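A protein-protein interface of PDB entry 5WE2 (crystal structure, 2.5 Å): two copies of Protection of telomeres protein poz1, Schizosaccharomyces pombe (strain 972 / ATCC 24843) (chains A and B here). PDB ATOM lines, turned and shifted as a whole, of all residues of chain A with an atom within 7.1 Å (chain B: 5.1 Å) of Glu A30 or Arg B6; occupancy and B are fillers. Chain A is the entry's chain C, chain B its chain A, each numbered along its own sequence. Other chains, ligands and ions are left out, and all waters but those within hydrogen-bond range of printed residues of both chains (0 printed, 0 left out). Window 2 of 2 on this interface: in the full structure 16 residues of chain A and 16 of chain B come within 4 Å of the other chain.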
ATOM      1  N   THR A  13     -22.321  36.999  16.611  1.00  0.00           N
ATOM      2  CA  THR A  13     -22.528  35.694  16.006  1.00  0.00           C
ATOM      3  C   THR A  13     -21.209  35.093  15.498  1.00  0.00           C
ATOM      4  O   THR A  13     -20.852  33.941  15.846  1.00  0.00           O
ATOM      5  CB  THR A  13     -23.544  35.787  14.877  1.00  0.00           C
ATOM      6  OG1 THR A  13     -24.805  36.205  15.435  1.00  0.00           O
ATOM      7  CG2 THR A  13     -23.684  34.424  14.167  1.00  0.00           C
ATOM      8  N   GLU A  15     -18.346  35.732  16.655  1.00  0.00           N
ATOM      9  CA  GLU A  15     -17.617  35.297  17.848  1.00  0.00           C
ATOM     10  C   GLU A  15     -18.040  33.904  18.253  1.00  0.00           C
ATOM     11  O   GLU A  15     -17.208  33.056  18.606  1.00  0.00           O
ATOM     12  CB  GLU A  15     -17.826  36.260  19.014  1.00  0.00           C
ATOM     13  CG  GLU A  15     -17.292  35.731  20.322  1.00  0.00           C
ATOM     14  CD  GLU A  15     -17.239  36.780  21.417  1.00  0.00           C
ATOM     15  OE1 GLU A  15     -17.006  36.398  22.592  1.00  0.00           O
ATOM     16  OE2 GLU A  15     -17.426  37.978  21.100  1.00  0.00           O
ATOM     17  N   THR A  16     -19.336  33.653  18.185  1.00  0.00           N
ATOM     18  CA  THR A  16     -19.824  32.308  18.475  1.00  0.00           C
ATOM     19  C   THR A  16     -19.293  31.228  17.499  1.00  0.00           C
ATOM     20  O   THR A  16     -19.128  30.068  17.870  1.00  0.00           O
ATOM     21  CB  THR A  16     -21.363  32.317  18.486  1.00  0.00           C
ATOM     22  OG1 THR A  16     -21.789  33.344  19.392  1.00  0.00           O
ATOM     23  CG2 THR A  16     -21.874  31.058  19.016  1.00  0.00           C
ATOM     24  N   PHE A  17     -19.030  31.592  16.248  1.00  0.00           N
ATOM     25  CA  PHE A  17     -18.541  30.596  15.295  1.00  0.00           C
ATOM     26  C   PHE A  17     -17.009  30.456  15.308  1.00  0.00           C
ATOM     27  O   PHE A  17     -16.471  29.430  14.897  1.00  0.00           O
ATOM     28  CB  PHE A  17     -18.991  30.936  13.866  1.00  0.00           C
ATOM     29  CG  PHE A  17     -20.430  30.602  13.576  1.00  0.00           C
ATOM     30  CD1 PHE A  17     -21.472  31.343  14.138  1.00  0.00           C
ATOM     31  CD2 PHE A  17     -20.745  29.569  12.702  1.00  0.00           C
ATOM     32  CE1 PHE A  17     -22.791  31.036  13.855  1.00  0.00           C
ATOM     33  CE2 PHE A  17     -22.071  29.260  12.409  1.00  0.00           C
ATOM     34  CZ  PHE A  17     -23.101  30.007  12.995  1.00  0.00           C
ATOM     35  N   PHE A  18     -16.318  31.493  15.776  1.00  0.00           N
ATOM     36  CA  PHE A  18     -14.877  31.620  15.577  1.00  0.00           C
ATOM     37  C   PHE A  18     -14.049  31.198  16.769  1.00  0.00           C
ATOM     38  O   PHE A  18     -12.965  30.632  16.597  1.00  0.00           O
ATOM     39  CB  PHE A  18     -14.509  33.057  15.229  1.00  0.00           C
ATOM     40  CG  PHE A  18     -14.652  33.381  13.792  1.00  0.00           C
ATOM     41  CD1 PHE A  18     -15.191  32.458  12.910  1.00  0.00           C
ATOM     42  CD2 PHE A  18     -14.214  34.594  13.305  1.00  0.00           C
ATOM     43  CE1 PHE A  18     -15.317  32.754  11.568  1.00  0.00           C
ATOM     44  CE2 PHE A  18     -14.339  34.900  11.961  1.00  0.00           C
ATOM     45  CZ  PHE A  18     -14.889  33.976  11.088  1.00  0.00           C
ATOM     46  N   LYS A  20     -12.809  28.973  19.457  1.00  0.00           N
ATOM     47  CA  LYS A  20     -12.756  27.530  19.595  1.00  0.00           C
ATOM     48  C   LYS A  20     -11.770  27.140  20.688  1.00  0.00           C
ATOM     49  O   LYS A  20     -10.706  27.745  20.809  1.00  0.00           O
ATOM     50  CB  LYS A  20     -12.350  26.886  18.257  1.00  0.00           C
ATOM     51  CG  LYS A  20     -13.430  25.982  17.670  1.00  0.00           C
ATOM     52  CD  LYS A  20     -14.654  26.740  17.200  1.00  0.00           C
ATOM     53  CE  LYS A  20     -15.738  25.773  16.758  1.00  0.00           C
ATOM     54  NZ  LYS A  20     -16.917  26.466  16.160  1.00  0.00           N
ATOM     55  N   TYR A  24      -9.811  27.112  15.027  1.00  0.00           N
ATOM     56  CA  TYR A  24     -10.966  27.269  14.167  1.00  0.00           C
ATOM     57  C   TYR A  24     -10.688  26.657  12.802  1.00  0.00           C
ATOM     58  O   TYR A  24      -9.646  26.881  12.205  1.00  0.00           O
ATOM     59  CB  TYR A  24     -11.359  28.742  14.010  1.00  0.00           C
ATOM     60  CG  TYR A  24     -12.421  28.921  12.973  1.00  0.00           C
ATOM     61  CD1 TYR A  24     -13.740  28.610  13.251  1.00  0.00           C
ATOM     62  CD2 TYR A  24     -12.105  29.364  11.696  1.00  0.00           C
ATOM     63  CE1 TYR A  24     -14.715  28.744  12.304  1.00  0.00           C
ATOM     64  CE2 TYR A  24     -13.084  29.509  10.735  1.00  0.00           C
ATOM     65  CZ  TYR A  24     -14.384  29.197  11.049  1.00  0.00           C
ATOM     66  OH  TYR A  24     -15.361  29.334  10.102  1.00  0.00           O
ATOM     67  N   ASP A  25     -11.626  25.862  12.324  1.00  0.00           N
ATOM     68  CA  ASP A  25     -11.653  25.510  10.918  1.00  0.00           C
ATOM     69  C   ASP A  25     -13.062  25.703  10.391  1.00  0.00           C
ATOM     70  O   ASP A  25     -14.034  25.594  11.137  1.00  0.00           O
ATOM     71  CB  ASP A  25     -11.212  24.076  10.670  1.00  0.00           C
ATOM     72  CG  ASP A  25     -11.183  23.746   9.188  1.00  0.00           C
ATOM     73  OD1 ASP A  25     -10.912  24.676   8.385  1.00  0.00           O
ATOM     74  OD2 ASP A  25     -11.460  22.580   8.824  1.00  0.00           O
ATOM     75  N   MET A  26     -13.183  25.974   9.104  1.00  0.00           N
ATOM     76  CA  MET A  26     -14.488  26.277   8.572  1.00  0.00           C
ATOM     77  C   MET A  26     -15.111  25.101   7.849  1.00  0.00           C
ATOM     78  O   MET A  26     -14.783  24.836   6.702  1.00  0.00           O
ATOM     79  CB  MET A  26     -14.409  27.467   7.636  1.00  0.00           C
ATOM     80  CG  MET A  26     -15.768  28.061   7.292  1.00  0.00           C
ATOM     81  SD  MET A  26     -15.580  28.813   5.693  1.00  0.00           S
ATOM     82  CE  MET A  26     -16.093  30.427   6.083  1.00  0.00           C
ATOM     83  N   GLN A  27     -16.029  24.434   8.544  1.00  0.00           N
ATOM     84  CA  GLN A  27     -16.880  23.386   8.003  1.00  0.00           C
ATOM     85  C   GLN A  27     -17.817  23.890   6.905  1.00  0.00           C
ATOM     86  O   GLN A  27     -18.274  25.033   6.964  1.00  0.00           O
ATOM     87  CB  GLN A  27     -17.720  22.779   9.127  1.00  0.00           C
ATOM     88  CG  GLN A  27     -17.127  22.936  10.508  1.00  0.00           C
ATOM     89  CD  GLN A  27     -15.985  21.967  10.767  1.00  0.00           C
ATOM     90  OE1 GLN A  27     -16.212  20.777  10.972  1.00  0.00           O
ATOM     91  NE2 GLN A  27     -14.753  22.474  10.773  1.00  0.00           N
ATOM     92  N   ARG A  28     -18.123  23.025   5.933  1.00  0.00           N
ATOM     93  CA  ARG A  28     -19.045  23.337   4.829  1.00  0.00           C
ATOM     94  C   ARG A  28     -20.391  23.903   5.300  1.00  0.00           C
ATOM     95  O   ARG A  28     -20.960  24.763   4.637  1.00  0.00           O
ATOM     96  CB  ARG A  28     -19.308  22.083   3.965  1.00  0.00           C
ATOM     97  CG  ARG A  28     -18.084  21.497   3.217  1.00  0.00           C
ATOM     98  CD  ARG A  28     -18.006  19.949   3.315  1.00  0.00           C
ATOM     99  NE  ARG A  28     -19.292  19.342   3.687  1.00  0.00           N
ATOM    100  CZ  ARG A  28     -19.460  18.453   4.670  1.00  0.00           C
ATOM    101  NH1 ARG A  28     -18.424  18.053   5.401  1.00  0.00           N
ATOM    102  NH2 ARG A  28     -20.676  17.971   4.932  1.00  0.00           N
ATOM    103  N   GLU A  29     -20.895  23.418   6.433  1.00  0.00           N
ATOM    104  CA  GLU A  29     -22.208  23.820   6.935  1.00  0.00           C
ATOM    105  C   GLU A  29     -22.265  25.282   7.417  1.00  0.00           C
ATOM    106  O   GLU A  29     -23.312  25.922   7.340  1.00  0.00           O
ATOM    107  CB  GLU A  29     -22.648  22.900   8.077  1.00  0.00           C
ATOM    108  CG  GLU A  29     -22.640  21.413   7.726  1.00  0.00           C
ATOM    109  CD  GLU A  29     -21.310  20.718   8.064  1.00  0.00           C
ATOM    110  OE1 GLU A  29     -20.256  21.394   8.106  1.00  0.00           O
ATOM    111  OE2 GLU A  29     -21.327  19.488   8.294  1.00  0.00           O
ATOM    112  N   GLU A  30     -21.148  25.800   7.920  1.00  0.00           N
ATOM    113  CA  GLU A  30     -21.090  27.181   8.391  1.00  0.00           C
ATOM    114  C   GLU A  30     -20.562  28.142   7.347  1.00  0.00           C
ATOM    115  O   GLU A  30     -20.445  29.326   7.606  1.00  0.00           O
ATOM    116  CB  GLU A  30     -20.196  27.316   9.609  1.00  0.00           C
ATOM    117  CG  GLU A  30     -20.420  26.320  10.697  1.00  0.00           C
ATOM    118  CD  GLU A  30     -19.294  26.384  11.684  1.00  0.00           C
ATOM    119  OE1 GLU A  30     -18.152  26.682  11.241  1.00  0.00           O
ATOM    120  OE2 GLU A  30     -19.546  26.146  12.885  1.00  0.00           O
ATOM    121  N   SER A  31     -20.198  27.636   6.184  1.00  0.00           N
ATOM    122  CA  SER A  31     -19.471  28.463   5.244  1.00  0.00           C
ATOM    123  C   SER A  31     -20.355  29.608   4.728  1.00  0.00           C
ATOM    124  O   SER A  31     -19.906  30.752   4.586  1.00  0.00           O
ATOM    125  CB  SER A  31     -18.920  27.592   4.102  1.00  0.00           C
ATOM    126  OG  SER A  31     -18.661  28.376   2.963  1.00  0.00           O
ATOM    127  N   SER A  32     -21.623  29.328   4.478  1.00  0.00           N
ATOM    128  CA  SER A  32     -22.505  30.374   3.955  1.00  0.00           C
ATOM    129  C   SER A  32     -22.784  31.488   4.989  1.00  0.00           C
ATOM    130  O   SER A  32     -22.795  32.677   4.662  1.00  0.00           O
ATOM    131  CB  SER A  32     -23.822  29.753   3.485  1.00  0.00           C
ATOM    132  OG  SER A  32     -24.778  30.763   3.128  1.00  0.00           O
ATOM    133  N   ILE A  33     -23.019  31.085   6.229  1.00  0.00           N
ATOM    134  CA  ILE A  33     -23.321  32.012   7.300  1.00  0.00           C
ATOM    135  C   ILE A  33     -22.064  32.830   7.687  1.00  0.00           C
ATOM    136  O   ILE A  33     -22.149  34.065   7.787  1.00  0.00           O
ATOM    137  CB  ILE A  33     -23.931  31.260   8.518  1.00  0.00           C
ATOM    138  CG1 ILE A  33     -24.529  32.243   9.539  1.00  0.00           C
ATOM    139  CG2 ILE A  33     -22.917  30.329   9.178  1.00  0.00           C
ATOM    140  CD1 ILE A  33     -25.632  33.084   8.988  1.00  0.00           C
ATOM    141  N   VAL A  34     -20.906  32.173   7.852  1.00  0.00           N
ATOM    142  CA  VAL A  34     -19.642  32.892   8.081  1.00  0.00           C
ATOM    143  C   VAL A  34     -19.344  33.843   6.924  1.00  0.00           C
ATOM    144  O   VAL A  34     -18.865  34.949   7.117  1.00  0.00           O
ATOM    145  CB  VAL A  34     -18.432  31.925   8.264  1.00  0.00           C
ATOM    146  CG1 VAL A  34     -17.150  32.681   8.254  1.00  0.00           C
ATOM    147  CG2 VAL A  34     -18.546  31.092   9.552  1.00  0.00           C
ATOM    148  N   ASN A  35     -19.639  33.434   5.703  1.00  0.00           N
ATOM    149  CA  ASN A  35     -19.359  34.316   4.578  1.00  0.00           C
ATOM    150  C   ASN A  35     -20.293  35.531   4.556  1.00  0.00           C
ATOM    151  O   ASN A  35     -19.875  36.660   4.273  1.00  0.00           O
ATOM    152  CB  ASN A  35     -19.430  33.527   3.254  1.00  0.00           C
ATOM    153  CG  ASN A  35     -18.123  32.784   2.952  1.00  0.00           C
ATOM    154  OD1 ASN A  35     -17.125  33.402   2.602  1.00  0.00           O
ATOM    155  ND2 ASN A  35     -18.122  31.469   3.117  1.00  0.00           N
ATOM    156  N   ALA A  36     -21.560  35.300   4.864  1.00  0.00           N
ATOM    157  CA  ALA A  36     -22.535  36.376   4.871  1.00  0.00           C
ATOM    158  C   ALA A  36     -22.194  37.383   5.966  1.00  0.00           C
ATOM    159  O   ALA A  36     -22.308  38.599   5.765  1.00  0.00           O
ATOM    160  CB  ALA A  36     -23.937  35.824   5.065  1.00  0.00           C
ATOM    161  N   ASN B   2     -22.749  23.300  21.434  1.00  0.00           N
ATOM    162  CA  ASN B   2     -22.164  24.424  20.713  1.00  0.00           C
ATOM    163  C   ASN B   2     -23.043  24.844  19.528  1.00  0.00           C
ATOM    164  O   ASN B   2     -23.183  26.053  19.250  1.00  0.00           O
ATOM    165  CB  ASN B   2     -20.746  24.089  20.231  1.00  0.00           C
ATOM    166  CG  ASN B   2     -19.701  24.205  21.343  1.00  0.00           C
ATOM    167  OD1 ASN B   2     -19.866  24.975  22.292  1.00  0.00           O
ATOM    168  ND2 ASN B   2     -18.615  23.442  21.218  1.00  0.00           N
ATOM    169  N   GLU B   3     -23.653  23.880  18.832  1.00  0.00           N
ATOM    170  CA  GLU B   3     -24.515  24.287  17.728  1.00  0.00           C
ATOM    171  C   GLU B   3     -25.720  25.030  18.290  1.00  0.00           C
ATOM    172  O   GLU B   3     -26.154  26.015  17.707  1.00  0.00           O
ATOM    173  CB  GLU B   3     -24.973  23.127  16.828  1.00  0.00           C
ATOM    174  CG  GLU B   3     -25.765  23.679  15.614  1.00  0.00           C
ATOM    175  CD  GLU B   3     -26.099  22.648  14.539  1.00  0.00           C
ATOM    176  OE1 GLU B   3     -26.569  21.545  14.900  1.00  0.00           O
ATOM    177  OE2 GLU B   3     -25.916  22.957  13.322  1.00  0.00           O
ATOM    178  N   LYS B   4     -26.213  24.599  19.443  1.00  0.00           N
ATOM    179  CA  LYS B   4     -27.320  25.298  20.099  1.00  0.00           C
ATOM    180  C   LYS B   4     -27.007  26.778  20.397  1.00  0.00           C
ATOM    181  O   LYS B   4     -27.758  27.667  19.990  1.00  0.00           O
ATOM    182  CB  LYS B   4     -27.705  24.577  21.387  1.00  0.00           C
ATOM    183  CG  LYS B   4     -28.952  25.133  22.055  1.00  0.00           C
ATOM    184  CD  LYS B   4     -30.141  25.098  21.112  1.00  0.00           C
ATOM    185  CE  LYS B   4     -31.444  25.323  21.856  1.00  0.00           C
ATOM    186  NZ  LYS B   4     -31.820  24.144  22.686  1.00  0.00           N
ATOM    187  N   ILE B   5     -25.892  27.024  21.088  1.00  0.00           N
ATOM    188  CA  ILE B   5     -25.377  28.371  21.358  1.00  0.00           C
ATOM    189  C   ILE B   5     -25.190  29.205  20.081  1.00  0.00           C
ATOM    190  O   ILE B   5     -25.607  30.373  20.020  1.00  0.00           O
ATOM    191  CB  ILE B   5     -24.022  28.307  22.117  1.00  0.00           C
ATOM    192  CG1 ILE B   5     -24.240  27.843  23.556  1.00  0.00           C
ATOM    193  CG2 ILE B   5     -23.326  29.660  22.125  1.00  0.00           C
ATOM    194  CD1 ILE B   5     -24.608  28.960  24.497  1.00  0.00           C
ATOM    195  N   ARG B   6     -24.594  28.601  19.061  1.00  0.00           N
ATOM    196  CA  ARG B   6     -24.464  29.245  17.748  1.00  0.00           C
ATOM    197  C   ARG B   6     -25.811  29.654  17.145  1.00  0.00           C
ATOM    198  O   ARG B   6     -25.972  30.761  16.628  1.00  0.00           O
ATOM    199  CB  ARG B   6     -23.711  28.315  16.790  1.00  0.00           C
ATOM    200  CG  ARG B   6     -22.218  28.589  16.773  1.00  0.00           C
ATOM    201  CD  ARG B   6     -21.372  27.360  16.681  1.00  0.00           C
ATOM    202  NE  ARG B   6     -21.649  26.586  15.480  1.00  0.00           N
ATOM    203  CZ  ARG B   6     -21.477  25.271  15.419  1.00  0.00           C
ATOM    204  NH1 ARG B   6     -21.027  24.629  16.494  1.00  0.00           N
ATOM    205  NH2 ARG B   6     -21.764  24.604  14.302  1.00  0.00           N
ATOM    206  N   SER B   7     -26.780  28.752  17.246  1.00  0.00           N
ATOM    207  CA  SER B   7     -28.116  28.979  16.733  1.00  0.00           C
ATOM    208  C   SER B   7     -28.815  30.107  17.456  1.00  0.00           C
ATOM    209  O   SER B   7     -29.438  30.965  16.819  1.00  0.00           O
ATOM    210  CB  SER B   7     -28.940  27.695  16.823  1.00  0.00           C
ATOM    211  OG  SER B   7     -28.562  26.817  15.775  1.00  0.00           O
ATOM    212  N   GLN B   8     -28.699  30.127  18.781  1.00  0.00           N
ATOM    213  CA  GLN B   8     -29.290  31.221  19.550  1.00  0.00           C
ATOM    214  C   GLN B   8     -28.636  32.518  19.158  1.00  0.00           C
ATOM    215  O   GLN B   8     -29.276  33.586  19.100  1.00  0.00           O
ATOM    216  CB  GLN B   8     -29.132  31.006  21.049  1.00  0.00           C
ATOM    217  CG  GLN B   8     -30.446  30.730  21.780  1.00  0.00           C
ATOM    218  CD  GLN B   8     -31.386  31.952  21.932  1.00  0.00           C
ATOM    219  OE1 GLN B   8     -31.023  33.118  21.692  1.00  0.00           O
ATOM    220  NE2 GLN B   8     -32.618  31.661  22.320  1.00  0.00           N
ATOM    221  N   SER B   9     -27.344  32.447  18.882  1.00  0.00           N
ATOM    222  CA  SER B   9     -26.681  33.673  18.488  1.00  0.00           C
ATOM    223  C   SER B   9     -27.249  34.167  17.140  1.00  0.00           C
ATOM    224  O   SER B   9     -27.460  35.375  16.951  1.00  0.00           O
ATOM    225  CB  SER B   9     -25.172  33.453  18.436  1.00  0.00           C
ATOM    226  OG  SER B   9     -24.506  34.681  18.258  1.00  0.00           O
ATOM    227  N   VAL B  10     -27.538  33.229  16.229  1.00  0.00           N
ATOM    228  CA  VAL B  10     -28.081  33.572  14.902  1.00  0.00           C
ATOM    229  C   VAL B  10     -29.504  34.183  15.023  1.00  0.00           C
ATOM    230  O   VAL B  10     -29.877  35.113  14.297  1.00  0.00           O
ATOM    231  CB  VAL B  10     -28.101  32.322  13.975  1.00  0.00           C
ATOM    232  CG1 VAL B  10     -28.889  32.570  12.688  1.00  0.00           C
ATOM    233  CG2 VAL B  10     -26.687  31.887  13.667  1.00  0.00           C
ATOM    234  N   TYR B  40     -29.196  28.449   8.046  1.00  0.00           N
ATOM    235  CA  TYR B  40     -28.504  27.783   9.150  1.00  0.00           C
ATOM    236  C   TYR B  40     -29.526  27.284  10.175  1.00  0.00           C
ATOM    237  O   TYR B  40     -29.471  26.142  10.583  1.00  0.00           O
ATOM    238  CB  TYR B  40     -27.499  28.729   9.801  1.00  0.00           C
ATOM    239  CG  TYR B  40     -26.644  28.045  10.822  1.00  0.00           C
ATOM    240  CD1 TYR B  40     -25.491  27.387  10.443  1.00  0.00           C
ATOM    241  CD2 TYR B  40     -26.991  28.045  12.173  1.00  0.00           C
ATOM    242  CE1 TYR B  40     -24.694  26.750  11.377  1.00  0.00           C
ATOM    243  CE2 TYR B  40     -26.194  27.420  13.116  1.00  0.00           C
ATOM    244  CZ  TYR B  40     -25.045  26.767  12.702  1.00  0.00           C
ATOM    245  OH  TYR B  40     -24.241  26.109  13.608  1.00  0.00           O
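The side-chain carboxylate (OE2) of Glu A30 is in salt-bridge range of the guanidinium group (NH2) of Arg B6 (3.1 Å). The backbone carbonyl oxygen of Ser B9 lies within hydrogen-bond range of the side-chain hydroxyl of Thr A13, at 3.2 Å. The side-chain hydroxyl (OG) of Ser B9 lies within hydrogen-bond range of the side-chain hydroxyl (OG1) of Thr A16 (3.2 Å).
The side-chain hydroxyl (OH) of Tyr B40 sits at hydrogen-bond distance from the guanidinium group (NH2) of Arg B6 (3.0 Å). The side-chain amino group (NZ) of Lys A20 lies within hydrogen-bond range of the backbone carbonyl oxygen (O) of Phe A17.
Among the printed residues, pairs that only touch across the chains: Thr A16 with Arg B6, Thr A16 with Ile B5, Phe A17 with Tyr B40, Phe A17 with Arg B6, Thr A13 with Val B10 and Phe A17 with Val B10.
Of chain B, only Arg B6 comes within 4 Å of Glu A30. Of chain A, only Thr A16, Phe A17 and Glu A30 come within 4 Å of Arg B6. Of the printed residues of chain B, Phe A17 touches Arg B6 (3.9 Å), Val B10 (3.99 Å) and Tyr B40 (3.8 Å). Of the printed residues of chain A, Val B10 touches Thr A13 and Phe A17. Printed residues of chain B within 4 Å of Thr A16: Ile B5 (3.7 Å), Arg B6 (3.4 Å) and Ser B9 (3.2 Å). Of the printed residues of chain A, Ile B5 touches Thr A16. Gln A27 touches none of the printed residues of chain B. The nearest residue of chain B that does not touch Glu A30 is Tyr B40 (4.3 Å). The nearest residue of chain A that does not touch Arg B6 is Lys A20 (4.5 Å).
Of the 19 printed residues of chain A, 4 touch a printed residue of chain B. Along chain A the printed residues that touch a printed residue of chain B span positions 13 to 30. Among the printed residues, 9 pairs touch across the chains. Among the printed residues, Asp or Glu carboxylates within 4 Å of a Lys or Arg side-chain nitrogen of the other chain: Glu A30 with Arg B6 (3.1 Å).
No position is printed for both chains. Of the 9 pairs that touch across the chains among the printed residues, none has its exchanged pair printed and touching as well.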
